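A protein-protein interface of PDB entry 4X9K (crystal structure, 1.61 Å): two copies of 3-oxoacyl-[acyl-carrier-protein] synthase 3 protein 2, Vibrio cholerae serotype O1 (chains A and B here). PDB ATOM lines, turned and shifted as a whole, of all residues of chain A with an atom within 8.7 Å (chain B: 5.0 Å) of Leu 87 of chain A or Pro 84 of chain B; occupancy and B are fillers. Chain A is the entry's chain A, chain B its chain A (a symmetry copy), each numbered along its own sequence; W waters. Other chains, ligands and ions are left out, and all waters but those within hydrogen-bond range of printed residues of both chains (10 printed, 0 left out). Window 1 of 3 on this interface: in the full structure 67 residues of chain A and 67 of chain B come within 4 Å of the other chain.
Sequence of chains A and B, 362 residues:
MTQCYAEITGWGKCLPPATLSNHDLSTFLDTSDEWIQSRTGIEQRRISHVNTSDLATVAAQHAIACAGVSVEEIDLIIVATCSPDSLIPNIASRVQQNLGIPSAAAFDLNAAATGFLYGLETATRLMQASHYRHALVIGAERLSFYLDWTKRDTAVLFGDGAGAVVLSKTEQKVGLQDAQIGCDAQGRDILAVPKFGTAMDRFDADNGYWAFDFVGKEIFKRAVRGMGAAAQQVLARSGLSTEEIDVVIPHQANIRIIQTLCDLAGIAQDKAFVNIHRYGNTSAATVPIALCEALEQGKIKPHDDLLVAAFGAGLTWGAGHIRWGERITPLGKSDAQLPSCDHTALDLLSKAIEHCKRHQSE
The backbone carbonyl oxygen (O) of Leu 87 of chain A lies within hydrogen-bond range of the side-chain amide nitrogen (ND2) of Asn 110 of chain B, at 2.8 Å. The backbone carbonyl oxygen of Phe 196 of chain B is in hydrogen-bond range of the backbone NH of Leu 87 of chain A. O of Asn 110 of chain B is in hydrogen-bond range of ND2 of Asn 90 of chain A (3.0 Å). The backbone carbonyl oxygen of Asp 108 of chain A lies within hydrogen-bond range of the backbone NH of Asn 110 of chain B, 2.9 Å away. N of Asn 110 of chain A sits at hydrogen-bond distance from O of Asp 108 of chain B (2.9 Å). The guanidinium group of Arg 188 of chain A sits at hydrogen-bond distance from the side-chain hydroxyl of Ser 86 of chain B, at 3.1 Å. The backbone NH of Leu 87 of chain B sits at hydrogen-bond distance from the backbone carbonyl oxygen of Phe 196 of chain A. The backbone carbonyl oxygen of Ser 83 of chain B is in hydrogen-bond range of the side-chain hydroxyl of Thr 198 of chain A (2.8 Å). N of Thr 198 of chain A lies within hydrogen-bond range of O of Asp 85 of chain B, 3.2 Å away. The backbone NH of Ala 199 of chain A sits at hydrogen-bond distance from the backbone carbonyl oxygen of Asp 85 of chain B (3.0 Å).
The backbone NH of Ile 91 of chain B lies within hydrogen-bond range of the side-chain carboxylate of Asp 108 of chain B (2.8 Å).
CG1 of Ile 88 of chain A touches SG of Cys 82 of chain B (3.9 Å). CA of Ser 86 of chain B touches O of Phe 196 of chain A, at 3.4 Å. Asp 85 of chain B touches Gly 197 of chain A (O to CA, 3.2 Å).
Of the printed residues of chain B, Pro 84 of chain A touches Leu 87 (3.9 Å) and Gly 197 (3.8 Å). Leu 87 of chain A touches five residues of chain B. Lys 195 of chain A touches none of the printed residues of chain B. Of chain A, only Thr 198 (2.8 Å) comes within 4 Å of Ser 83 of chain B. Of chain A, only Leu 87 (3.9 Å), Gly 197 (3.8 Å) and Thr 198 (2.9 Å) come within 4 Å of Pro 84 of chain B. The nearest residue of chain A that does not touch Pro 84 of chain B is Ala 199 of chain A (4.6 Å). The nearest printed residue of chain B that does not touch Asp 108 of chain A is Thr 81 of chain B (6.8 Å).
Printed residues of chain B that touch a printed residue of chain A: Thr 52, Cys 82, Ser 83, Pro 84, Asp 85, Ser 86, Leu 87, Asp 108, Asn 110, Tyr 146, Phe 196 and Gly 197. Hydrophobic or aromatic side chains of chain B that line the printed part of chain A: Pro 84, Leu 87, Tyr 146 and Phe 196. Among the printed residues, 34 pairs touch across the chains. Among the printed residues, no Asp or Glu carboxylate lies within 4 Å of a Lys or Arg side-chain nitrogen of the other chain.
Pro 84 of chain A touches Gly 197 of chain B, and with the chains exchanged Gly 197 of chain A touches Pro 84 of chain B. Phe 196 of chain A touches Gly 197 of chain B, and with the chains exchanged Gly 197 of chain A touches Phe 196 of chain B.
Water W7 lies within hydrogen-bond range of O of Phe 196 of chain B (2.8 Å), N of Ile 88 of chain A (2.9 Å) and N of Leu 87 of chain A (3.0 Å).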
ATOM      1  N   THR A  81     -11.414 -25.365 -18.363  1.00  0.00           N
ATOM      2  CA  THR A  81     -10.132 -25.879 -17.846  1.00  0.00           C
ATOM      3  C   THR A  81      -9.051 -25.667 -18.887  1.00  0.00           C
ATOM      4  O   THR A  81      -9.332 -25.655 -20.103  1.00  0.00           O
ATOM      5  CB  THR A  81     -10.206 -27.383 -17.457  1.00  0.00           C
ATOM      6  OG1 THR A  81      -8.988 -27.779 -16.789  1.00  0.00           O
ATOM      7  CG2 THR A  81     -10.399 -28.275 -18.667  1.00  0.00           C
ATOM      8  N   CYS A  82      -7.816 -25.516 -18.399  1.00  0.00           N
ATOM      9  CA  CYS A  82      -6.630 -25.580 -19.232  1.00  0.00           C
ATOM     10  C   CYS A  82      -5.676 -26.705 -18.763  1.00  0.00           C
ATOM     11  O   CYS A  82      -4.532 -26.805 -19.252  1.00  0.00           O
ATOM     12  CB  CYS A  82      -5.916 -24.233 -19.281  1.00  0.00           C
ATOM     13  SG  CYS A  82      -5.175 -23.744 -17.707  1.00  0.00           S
ATOM     14  N   SER A  83      -6.182 -27.563 -17.880  1.00  0.00           N
ATOM     15  CA  SER A  83      -5.411 -28.663 -17.282  1.00  0.00           C
ATOM     16  C   SER A  83      -6.196 -29.978 -17.281  1.00  0.00           C
ATOM     17  O   SER A  83      -6.245 -30.700 -16.281  1.00  0.00           O
ATOM     18  CB  SER A  83      -4.989 -28.261 -15.850  1.00  0.00           C
ATOM     19  OG  SER A  83      -6.097 -27.908 -15.030  1.00  0.00           O
ATOM     20  N   PRO A  84      -6.839 -30.321 -18.415  1.00  0.00           N
ATOM     21  CA  PRO A  84      -7.681 -31.514 -18.409  1.00  0.00           C
ATOM     22  C   PRO A  84      -6.905 -32.832 -18.255  1.00  0.00           C
ATOM     23  O   PRO A  84      -5.836 -32.945 -18.811  1.00  0.00           O
ATOM     24  CB  PRO A  84      -8.328 -31.481 -19.797  1.00  0.00           C
ATOM     25  CG  PRO A  84      -7.298 -30.807 -20.642  1.00  0.00           C
ATOM     26  CD  PRO A  84      -6.708 -29.738 -19.759  1.00  0.00           C
ATOM     27  N   ASP A  85      -7.485 -33.787 -17.546  1.00  0.00           N
ATOM     28  CA  ASP A  85      -6.928 -35.153 -17.439  1.00  0.00           C
ATOM     29  C   ASP A  85      -6.460 -35.674 -18.803  1.00  0.00           C
ATOM     30  O   ASP A  85      -5.350 -36.239 -18.955  1.00  0.00           O
ATOM     31  CB  ASP A  85      -7.973 -36.163 -16.988  1.00  0.00           C
ATOM     32  CG  ASP A  85      -8.711 -35.808 -15.726  1.00  0.00           C
ATOM     33  OD1 ASP A  85      -8.823 -34.630 -15.313  1.00  0.00           O
ATOM     34  OD2 ASP A  85      -9.297 -36.782 -15.202  1.00  0.00           O
ATOM     35  N   SER A  86      -7.363 -35.545 -19.771  1.00  0.00           N
ATOM     36  CA  SER A  86      -7.184 -36.070 -21.119  1.00  0.00           C
ATOM     37  C   SER A  86      -7.720 -35.073 -22.119  1.00  0.00           C
ATOM     38  O   SER A  86      -8.534 -34.189 -21.783  1.00  0.00           O
ATOM     39  CB  SER A  86      -7.931 -37.408 -21.300  1.00  0.00           C
ATOM     40  OG  SER A  86      -9.308 -37.298 -20.954  1.00  0.00           O
ATOM     41  N   LEU A  87      -7.240 -35.228 -23.347  1.00  0.00           N
ATOM     42  CA  LEU A  87      -7.777 -34.534 -24.517  1.00  0.00           C
ATOM     43  C   LEU A  87      -8.759 -35.417 -25.298  1.00  0.00           C
ATOM     44  O   LEU A  87      -9.732 -34.916 -25.891  1.00  0.00           O
ATOM     45  CB  LEU A  87      -6.649 -34.066 -25.433  1.00  0.00           C
ATOM     46  CG  LEU A  87      -5.882 -32.790 -25.076  1.00  0.00           C
ATOM     47  CD1 LEU A  87      -6.792 -31.568 -25.173  1.00  0.00           C
ATOM     48  CD2 LEU A  87      -5.168 -32.867 -23.731  1.00  0.00           C
ATOM     49  N   ILE A  88      -8.513 -36.724 -25.298  1.00  0.00           N
ATOM     50  CA  ILE A  88      -9.425 -37.667 -25.930  1.00  0.00           C
ATOM     51  C   ILE A  88      -9.846 -38.683 -24.883  1.00  0.00           C
ATOM     52  O   ILE A  88      -8.981 -39.448 -24.416  1.00  0.00           O
ATOM     53  CB  ILE A  88      -8.747 -38.422 -27.096  1.00  0.00           C
ATOM     54  CG1 ILE A  88      -8.208 -37.437 -28.146  1.00  0.00           C
ATOM     55  CG2 ILE A  88      -9.744 -39.381 -27.744  1.00  0.00           C
ATOM     56  CD1 ILE A  88      -7.434 -38.083 -29.286  1.00  0.00           C
ATOM     57  N   PRO A  89     -11.105 -38.709 -24.445  1.00  0.00           N
ATOM     58  CA  PRO A  89     -12.118 -37.693 -24.675  1.00  0.00           C
ATOM     59  C   PRO A  89     -11.919 -36.505 -23.741  1.00  0.00           C
ATOM     60  O   PRO A  89     -10.908 -36.409 -23.020  1.00  0.00           O
ATOM     61  CB  PRO A  89     -13.435 -38.397 -24.281  1.00  0.00           C
ATOM     62  CG  PRO A  89     -13.053 -39.777 -23.875  1.00  0.00           C
ATOM     63  CD  PRO A  89     -11.615 -39.750 -23.545  1.00  0.00           C
ATOM     64  N   ASN A  90     -12.870 -35.583 -23.804  1.00  0.00           N
ATOM     65  CA  ASN A  90     -12.885 -34.438 -22.921  1.00  0.00           C
ATOM     66  C   ASN A  90     -13.172 -34.864 -21.483  1.00  0.00           C
ATOM     67  O   ASN A  90     -13.496 -36.037 -21.229  1.00  0.00           O
ATOM     68  CB  ASN A  90     -13.884 -33.395 -23.446  1.00  0.00           C
ATOM     69  CG  ASN A  90     -15.332 -33.820 -23.332  1.00  0.00           C
ATOM     70  OD1 ASN A  90     -15.710 -34.651 -22.507  1.00  0.00           O
ATOM     71  ND2 ASN A  90     -16.169 -33.222 -24.167  1.00  0.00           N
ATOM     72  N   ILE A  91     -13.009 -33.954 -20.520  1.00  0.00           N
ATOM     73  CA  ILE A  91     -13.340 -34.289 -19.146  1.00  0.00           C
ATOM     74  C   ILE A  91     -14.738 -33.911 -18.700  1.00  0.00           C
ATOM     75  O   ILE A  91     -15.219 -34.436 -17.710  1.00  0.00           O
ATOM     76  CB  ILE A  91     -12.270 -33.843 -18.118  1.00  0.00           C
ATOM     77  CG1 ILE A  91     -12.170 -32.327 -17.989  1.00  0.00           C
ATOM     78  CG2 ILE A  91     -10.932 -34.484 -18.472  1.00  0.00           C
ATOM     79  CD1 ILE A  91     -11.562 -31.886 -16.675  1.00  0.00           C
ATOM     80  N   SER A  93     -17.263 -35.048 -20.171  1.00  0.00           N
ATOM     81  CA  SER A  93     -17.839 -36.397 -20.267  1.00  0.00           C
ATOM     82  C   SER A  93     -17.459 -37.278 -19.081  1.00  0.00           C
ATOM     83  O   SER A  93     -18.224 -38.185 -18.770  1.00  0.00           O
ATOM     84  CB  SER A  93     -17.446 -37.116 -21.563  1.00  0.00           C
ATOM     85  OG  SER A  93     -16.048 -37.293 -21.687  1.00  0.00           O
ATOM     86  N   ASP A 108     -15.487 -29.390 -23.069  1.00  0.00           N
ATOM     87  CA  ASP A 108     -14.486 -28.614 -22.344  1.00  0.00           C
ATOM     88  C   ASP A 108     -14.252 -27.320 -23.118  1.00  0.00           C
ATOM     89  O   ASP A 108     -14.219 -27.306 -24.360  1.00  0.00           O
ATOM     90  CB  ASP A 108     -13.152 -29.367 -22.207  1.00  0.00           C
ATOM     91  CG  ASP A 108     -13.260 -30.640 -21.393  1.00  0.00           C
ATOM     92  OD1 ASP A 108     -14.329 -30.902 -20.816  1.00  0.00           O
ATOM     93  OD2 ASP A 108     -12.259 -31.407 -21.348  1.00  0.00           O
ATOM     94  N   ASN A 110     -11.708 -23.986 -23.276  1.00  0.00           N
ATOM     95  CA  ASN A 110     -10.414 -23.437 -22.863  1.00  0.00           C
ATOM     96  C   ASN A 110     -10.282 -21.961 -23.216  1.00  0.00           C
ATOM     97  O   ASN A 110     -10.110 -21.618 -24.379  1.00  0.00           O
ATOM     98  CB  ASN A 110      -9.245 -24.198 -23.468  1.00  0.00           C
ATOM     99  CG  ASN A 110      -7.906 -23.762 -22.879  1.00  0.00           C
ATOM    100  OD1 ASN A 110      -7.851 -22.915 -21.968  1.00  0.00           O
ATOM    101  ND2 ASN A 110      -6.829 -24.306 -23.417  1.00  0.00           N
ATOM    102  N   TYR A 146       1.845 -28.251 -14.113  1.00  0.00           N
ATOM    103  CA  TYR A 146       2.630 -27.488 -15.080  1.00  0.00           C
ATOM    104  C   TYR A 146       3.900 -26.821 -14.563  1.00  0.00           C
ATOM    105  O   TYR A 146       4.715 -26.354 -15.368  1.00  0.00           O
ATOM    106  CB  TYR A 146       1.768 -26.366 -15.658  1.00  0.00           C
ATOM    107  CG  TYR A 146       0.716 -26.816 -16.633  1.00  0.00           C
ATOM    108  CD1 TYR A 146       1.081 -27.315 -17.876  1.00  0.00           C
ATOM    109  CD2 TYR A 146      -0.642 -26.727 -16.335  1.00  0.00           C
ATOM    110  CE1 TYR A 146       0.129 -27.721 -18.790  1.00  0.00           C
ATOM    111  CE2 TYR A 146      -1.608 -27.138 -17.250  1.00  0.00           C
ATOM    112  CZ  TYR A 146      -1.220 -27.646 -18.466  1.00  0.00           C
ATOM    113  OH  TYR A 146      -2.160 -28.038 -19.406  1.00  0.00           O
ATOM    114  N   ARG A 188      -0.533 -12.839 -26.290  1.00  0.00           N
ATOM    115  CA  ARG A 188      -0.502 -14.290 -26.238  1.00  0.00           C
ATOM    116  C   ARG A 188       0.792 -14.877 -25.655  1.00  0.00           C
ATOM    117  O   ARG A 188       0.781 -15.944 -25.025  1.00  0.00           O
ATOM    118  CB  ARG A 188      -0.800 -14.910 -27.631  1.00  0.00           C
ATOM    119  CG  ARG A 188      -1.116 -16.391 -27.578  1.00  0.00           C
ATOM    120  CD  ARG A 188      -1.511 -17.020 -28.918  1.00  0.00           C
ATOM    121  NE  ARG A 188      -1.825 -18.417 -28.649  1.00  0.00           N
ATOM    122  CZ  ARG A 188      -0.966 -19.429 -28.605  1.00  0.00           C
ATOM    123  NH1 ARG A 188       0.317 -19.269 -28.918  1.00  0.00           N
ATOM    124  NH2 ARG A 188      -1.393 -20.639 -28.270  1.00  0.00           N
ATOM    125  N   VAL A 193       2.639 -21.745 -21.711  1.00  0.00           N
ATOM    126  CA  VAL A 193       3.429 -22.975 -21.666  1.00  0.00           C
ATOM    127  C   VAL A 193       3.414 -23.544 -23.097  1.00  0.00           C
ATOM    128  O   VAL A 193       2.640 -24.446 -23.405  1.00  0.00           O
ATOM    129  CB  VAL A 193       2.902 -23.999 -20.625  1.00  0.00           C
ATOM    130  CG1 VAL A 193       3.798 -25.224 -20.568  1.00  0.00           C
ATOM    131  CG2 VAL A 193       2.792 -23.368 -19.245  1.00  0.00           C
ATOM    132  N   PRO A 194       4.259 -22.986 -23.987  1.00  0.00           N
ATOM    133  CA  PRO A 194       4.150 -23.355 -25.402  1.00  0.00           C
ATOM    134  C   PRO A 194       4.415 -24.831 -25.707  1.00  0.00           C
ATOM    135  O   PRO A 194       3.923 -25.317 -26.712  1.00  0.00           O
ATOM    136  CB  PRO A 194       5.184 -22.452 -26.090  1.00  0.00           C
ATOM    137  CG  PRO A 194       5.296 -21.288 -25.171  1.00  0.00           C
ATOM    138  CD  PRO A 194       5.197 -21.871 -23.790  1.00  0.00           C
ATOM    139  N   LYS A 195       5.137 -25.550 -24.841  1.00  0.00           N
ATOM    140  CA  LYS A 195       5.534 -26.936 -25.145  1.00  0.00           C
ATOM    141  C   LYS A 195       4.918 -28.007 -24.235  1.00  0.00           C
ATOM    142  O   LYS A 195       5.508 -29.073 -23.996  1.00  0.00           O
ATOM    143  CB  LYS A 195       7.062 -27.040 -25.177  1.00  0.00           C
ATOM    144  CG  LYS A 195       7.703 -26.163 -26.238  1.00  0.00           C
ATOM    145  CD  LYS A 195       7.300 -26.559 -27.650  1.00  0.00           C
ATOM    146  CE  LYS A 195       8.121 -25.795 -28.679  1.00  0.00           C
ATOM    147  NZ  LYS A 195       7.656 -26.061 -30.067  1.00  0.00           N
ATOM    148  N   PHE A 196       3.691 -27.758 -23.771  1.00  0.00           N
ATOM    149  CA  PHE A 196       2.828 -28.849 -23.378  1.00  0.00           C
ATOM    150  C   PHE A 196       1.597 -28.797 -24.271  1.00  0.00           C
ATOM    151  O   PHE A 196       0.828 -27.829 -24.232  1.00  0.00           O
ATOM    152  CB  PHE A 196       2.376 -28.835 -21.919  1.00  0.00           C
ATOM    153  CG  PHE A 196       1.495 -30.012 -21.607  1.00  0.00           C
ATOM    154  CD1 PHE A 196       2.040 -31.287 -21.506  1.00  0.00           C
ATOM    155  CD2 PHE A 196       0.105 -29.884 -21.579  1.00  0.00           C
ATOM    156  CE1 PHE A 196       1.243 -32.388 -21.284  1.00  0.00           C
ATOM    157  CE2 PHE A 196      -0.691 -30.988 -21.381  1.00  0.00           C
ATOM    158  CZ  PHE A 196      -0.140 -32.239 -21.226  1.00  0.00           C
ATOM    159  N   GLY A 197       1.415 -29.855 -25.049  1.00  0.00           N
ATOM    160  CA  GLY A 197       0.360 -29.941 -26.054  1.00  0.00           C
ATOM    161  C   GLY A 197       0.936 -30.631 -27.269  1.00  0.00           C
ATOM    162  O   GLY A 197       2.016 -31.206 -27.180  1.00  0.00           O
ATOM    163  N   THR A 198       0.245 -30.585 -28.405  1.00  0.00           N
ATOM    164  CA  THR A 198       0.750 -31.291 -29.590  1.00  0.00           C
ATOM    165  C   THR A 198       1.929 -30.571 -30.256  1.00  0.00           C
ATOM    166  O   THR A 198       2.487 -31.098 -31.217  1.00  0.00           O
ATOM    167  CB  THR A 198      -0.365 -31.586 -30.633  1.00  0.00           C
ATOM    168  OG1 THR A 198      -0.843 -30.356 -31.196  1.00  0.00           O
ATOM    169  CG2 THR A 198      -1.518 -32.343 -29.980  1.00  0.00           C
ATOM    170  N   ALA A 199       2.308 -29.397 -29.765  1.00  0.00           N
ATOM    171  CA  ALA A 199       3.538 -28.719 -30.190  1.00  0.00           C
ATOM    172  C   ALA A 199       4.780 -29.414 -29.611  1.00  0.00           C
ATOM    173  O   ALA A 199       5.887 -29.183 -30.099  1.00  0.00           O
ATOM    174  CB  ALA A 199       3.537 -27.249 -29.781  1.00  0.00           C
ATOM    175  N   MET A 200       4.611 -30.233 -28.578  1.00  0.00           N
ATOM    176  CA  MET A 200       5.756 -30.833 -27.887  1.00  0.00           C
ATOM    177  C   MET A 200       6.234 -32.034 -28.679  1.00  0.00           C
ATOM    178  O   MET A 200       5.498 -32.579 -29.507  1.00  0.00           O
ATOM    179  CB  MET A 200       5.398 -31.242 -26.453  1.00  0.00           C
ATOM    180  CG  MET A 200       4.646 -32.552 -26.309  1.00  0.00           C
ATOM    181  SD  MET A 200       3.760 -32.728 -24.741  1.00  0.00           S
ATOM    182  CE  MET A 200       5.112 -32.692 -23.553  1.00  0.00           C
ATOM    183  N   THR B  52      -1.316 -27.802 -35.449  1.00  0.00           N
ATOM    184  CA  THR B  52      -2.759 -27.663 -35.606  1.00  0.00           C
ATOM    185  C   THR B  52      -3.188 -26.235 -35.880  1.00  0.00           C
ATOM    186  O   THR B  52      -3.986 -25.986 -36.776  1.00  0.00           O
ATOM    187  CB  THR B  52      -3.465 -28.172 -34.343  1.00  0.00           C
ATOM    188  OG1 THR B  52      -3.033 -29.518 -34.090  1.00  0.00           O
ATOM    189  CG2 THR B  52      -4.990 -28.138 -34.520  1.00  0.00           C
ATOM    190  N   THR B  81     -11.188 -28.617 -31.363  1.00  0.00           N
ATOM    191  CA  THR B  81      -9.980 -29.450 -31.500  1.00  0.00           C
ATOM    192  C   THR B  81      -9.834 -30.327 -30.272  1.00  0.00           C
ATOM    193  O   THR B  81     -10.272 -29.950 -29.165  1.00  0.00           O
ATOM    194  CB  THR B  81      -8.691 -28.604 -31.704  1.00  0.00           C
ATOM    195  OG1 THR B  81      -7.577 -29.470 -32.016  1.00  0.00           O
ATOM    196  CG2 THR B  81      -8.339 -27.798 -30.469  1.00  0.00           C
ATOM    197  N   CYS B  82      -9.203 -31.487 -30.475  1.00  0.00           N
ATOM    198  CA  CYS B  82      -8.727 -32.322 -29.388  1.00  0.00           C
ATOM    199  C   CYS B  82      -7.198 -32.540 -29.477  1.00  0.00           C
ATOM    200  O   CYS B  82      -6.635 -33.365 -28.728  1.00  0.00           O
ATOM    201  CB  CYS B  82      -9.475 -33.651 -29.344  1.00  0.00           C
ATOM    202  SG  CYS B  82      -9.127 -34.730 -30.752  1.00  0.00           S
ATOM    203  N   SER B  83      -6.551 -31.760 -30.340  1.00  0.00           N
ATOM    204  CA  SER B  83      -5.106 -31.858 -30.599  1.00  0.00           C
ATOM    205  C   SER B  83      -4.433 -30.482 -30.617  1.00  0.00           C
ATOM    206  O   SER B  83      -3.632 -30.167 -31.503  1.00  0.00           O
ATOM    207  CB  SER B  83      -4.885 -32.608 -31.933  1.00  0.00           C
ATOM    208  OG  SER B  83      -5.562 -31.995 -33.025  1.00  0.00           O
ATOM    209  N   PRO B  84      -4.748 -29.621 -29.629  1.00  0.00           N
ATOM    210  CA  PRO B  84      -4.203 -28.267 -29.680  1.00  0.00           C
ATOM    211  C   PRO B  84      -2.681 -28.193 -29.484  1.00  0.00           C
ATOM    212  O   PRO B  84      -2.162 -28.940 -28.685  1.00  0.00           O
ATOM    213  CB  PRO B  84      -4.888 -27.580 -28.496  1.00  0.00           C
ATOM    214  CG  PRO B  84      -5.104 -28.694 -27.527  1.00  0.00           C
ATOM    215  CD  PRO B  84      -5.471 -29.884 -28.375  1.00  0.00           C
ATOM    216  N   ASP B  85      -2.032 -27.275 -30.182  1.00  0.00           N
ATOM    217  CA  ASP B  85      -0.594 -26.989 -29.985  1.00  0.00           C
ATOM    218  C   ASP B  85      -0.239 -26.913 -28.495  1.00  0.00           C
ATOM    219  O   ASP B  85       0.767 -27.493 -28.019  1.00  0.00           O
ATOM    220  CB  ASP B  85      -0.203 -25.625 -30.535  1.00  0.00           C
ATOM    221  CG  ASP B  85      -0.585 -25.373 -31.968  1.00  0.00           C
ATOM    222  OD1 ASP B  85      -1.516 -25.988 -32.541  1.00  0.00           O
ATOM    223  OD2 ASP B  85       0.032 -24.417 -32.488  1.00  0.00           O
ATOM    224  N   SER B  86      -1.039 -26.120 -27.787  1.00  0.00           N
ATOM    225  CA  SER B  86      -0.828 -25.807 -26.380  1.00  0.00           C
ATOM    226  C   SER B  86      -2.158 -25.794 -25.664  1.00  0.00           C
ATOM    227  O   SER B  86      -3.230 -25.658 -26.289  1.00  0.00           O
ATOM    228  CB  SER B  86      -0.157 -24.427 -26.210  1.00  0.00           C
ATOM    229  OG  SER B  86      -0.883 -23.399 -26.877  1.00  0.00           O
ATOM    230  N   LEU B  87      -2.067 -25.948 -24.349  1.00  0.00           N
ATOM    231  CA  LEU B  87      -3.188 -25.745 -23.432  1.00  0.00           C
ATOM    232  C   LEU B  87      -3.153 -24.349 -22.796  1.00  0.00           C
ATOM    233  O   LEU B  87      -4.207 -23.753 -22.512  1.00  0.00           O
ATOM    234  CB  LEU B  87      -3.199 -26.818 -22.346  1.00  0.00           C
ATOM    235  CG  LEU B  87      -3.766 -28.202 -22.672  1.00  0.00           C
ATOM    236  CD1 LEU B  87      -5.266 -28.119 -22.943  1.00  0.00           C
ATOM    237  CD2 LEU B  87      -3.020 -28.915 -23.794  1.00  0.00           C
ATOM    238  N   ILE B  91      -5.456 -22.267 -28.574  1.00  0.00           N
ATOM    239  CA  ILE B  91      -5.033 -21.982 -29.934  1.00  0.00           C
ATOM    240  C   ILE B  91      -5.967 -21.097 -30.736  1.00  0.00           C
ATOM    241  O   ILE B  91      -5.556 -20.535 -31.737  1.00  0.00           O
ATOM    242  CB  ILE B  91      -4.605 -23.238 -30.733  1.00  0.00           C
ATOM    243  CG1 ILE B  91      -5.770 -24.178 -31.025  1.00  0.00           C
ATOM    244  CG2 ILE B  91      -3.465 -23.937 -30.001  1.00  0.00           C
ATOM    245  CD1 ILE B  91      -5.512 -25.088 -32.207  1.00  0.00           C
ATOM    246  N   ASP B 108     -11.088 -22.443 -27.264  1.00  0.00           N
ATOM    247  CA  ASP B 108     -11.038 -23.788 -27.828  1.00  0.00           C
ATOM    248  C   ASP B 108     -12.159 -24.601 -27.190  1.00  0.00           C
ATOM    249  O   ASP B 108     -12.442 -24.481 -25.986  1.00  0.00           O
ATOM    250  CB  ASP B 108      -9.693 -24.484 -27.556  1.00  0.00           C
ATOM    251  CG  ASP B 108      -8.514 -23.790 -28.207  1.00  0.00           C
ATOM    252  OD1 ASP B 108      -8.719 -22.838 -28.979  1.00  0.00           O
ATOM    253  OD2 ASP B 108      -7.352 -24.194 -27.921  1.00  0.00           O
ATOM    254  N   ASN B 110     -13.615 -28.524 -26.866  1.00  0.00           N
ATOM    255  CA  ASN B 110     -13.298 -29.944 -27.033  1.00  0.00           C
ATOM    256  C   ASN B 110     -14.525 -30.827 -26.847  1.00  0.00           C
ATOM    257  O   ASN B 110     -14.988 -31.014 -25.729  1.00  0.00           O
ATOM    258  CB  ASN B 110     -12.206 -30.407 -26.082  1.00  0.00           C
ATOM    259  CG  ASN B 110     -11.732 -31.824 -26.394  1.00  0.00           C
ATOM    260  OD1 ASN B 110     -12.188 -32.454 -27.367  1.00  0.00           O
ATOM    261  ND2 ASN B 110     -10.849 -32.340 -25.557  1.00  0.00           N
ATOM    262  N   TYR B 146      -0.939 -38.450 -32.024  1.00  0.00           N
ATOM    263  CA  TYR B 146      -1.383 -39.398 -31.005  1.00  0.00           C
ATOM    264  C   TYR B 146      -1.152 -40.878 -31.292  1.00  0.00           C
ATOM    265  O   TYR B 146      -1.299 -41.706 -30.386  1.00  0.00           O
ATOM    266  CB  TYR B 146      -2.888 -39.240 -30.788  1.00  0.00           C
ATOM    267  CG  TYR B 146      -3.291 -38.003 -30.035  1.00  0.00           C
ATOM    268  CD1 TYR B 146      -2.979 -37.869 -28.689  1.00  0.00           C
ATOM    269  CD2 TYR B 146      -4.000 -36.973 -30.649  1.00  0.00           C
ATOM    270  CE1 TYR B 146      -3.352 -36.747 -27.977  1.00  0.00           C
ATOM    271  CE2 TYR B 146      -4.376 -35.835 -29.939  1.00  0.00           C
ATOM    272  CZ  TYR B 146      -4.040 -35.721 -28.612  1.00  0.00           C
ATOM    273  OH  TYR B 146      -4.424 -34.611 -27.875  1.00  0.00           O
ATOM    274  N   PHE B 196      -2.627 -39.030 -22.341  1.00  0.00           N
ATOM    275  CA  PHE B 196      -2.087 -37.764 -22.784  1.00  0.00           C
ATOM    276  C   PHE B 196      -2.976 -36.669 -22.215  1.00  0.00           C
ATOM    277  O   PHE B 196      -4.163 -36.579 -22.553  1.00  0.00           O
ATOM    278  CB  PHE B 196      -1.994 -37.583 -24.298  1.00  0.00           C
ATOM    279  CG  PHE B 196      -1.412 -36.245 -24.655  1.00  0.00           C
ATOM    280  CD1 PHE B 196      -0.057 -35.997 -24.466  1.00  0.00           C
ATOM    281  CD2 PHE B 196      -2.233 -35.177 -25.021  1.00  0.00           C
ATOM    282  CE1 PHE B 196       0.485 -34.759 -24.727  1.00  0.00           C
ATOM    283  CE2 PHE B 196      -1.693 -33.934 -25.258  1.00  0.00           C
ATOM    284  CZ  PHE B 196      -0.342 -33.712 -25.123  1.00  0.00           C
ATOM    285  N   GLY B 197      -2.382 -35.834 -21.373  1.00  0.00           N
ATOM    286  CA  GLY B 197      -3.093 -34.792 -20.638  1.00  0.00           C
ATOM    287  C   GLY B 197      -2.507 -34.730 -19.246  1.00  0.00           C
ATOM    288  O   GLY B 197      -1.452 -35.311 -19.009  1.00  0.00           O
HETATM  289  O   HOH W   1       1.702 -21.778 -28.281  1.00  0.00           O
HETATM  290  O   HOH W   2     -12.057 -35.324 -27.314  1.00  0.00           O
HETATM  291  O   HOH W   3       0.353 -25.621 -22.656  1.00  0.00           O
HETATM  292  O   HOH W   4      -5.411 -21.436 -21.628  1.00  0.00           O
HETATM  293  O   HOH W   5      -6.191 -25.707 -25.932  1.00  0.00           O
HETATM  294  O   HOH W   6     -11.251 -27.019 -24.855  1.00  0.00           O
HETATM  295  O   HOH W   7      -5.860 -37.612 -24.460  1.00  0.00           O
HETATM  296  O   HOH W   8       0.682 -21.920 -31.101  1.00  0.00           O
HETATM  297  O   HOH W   9      -9.950 -31.771 -22.807  1.00  0.00           O
HETATM  298  O   HOH W  10       0.368 -29.612 -33.487  1.00  0.00           O
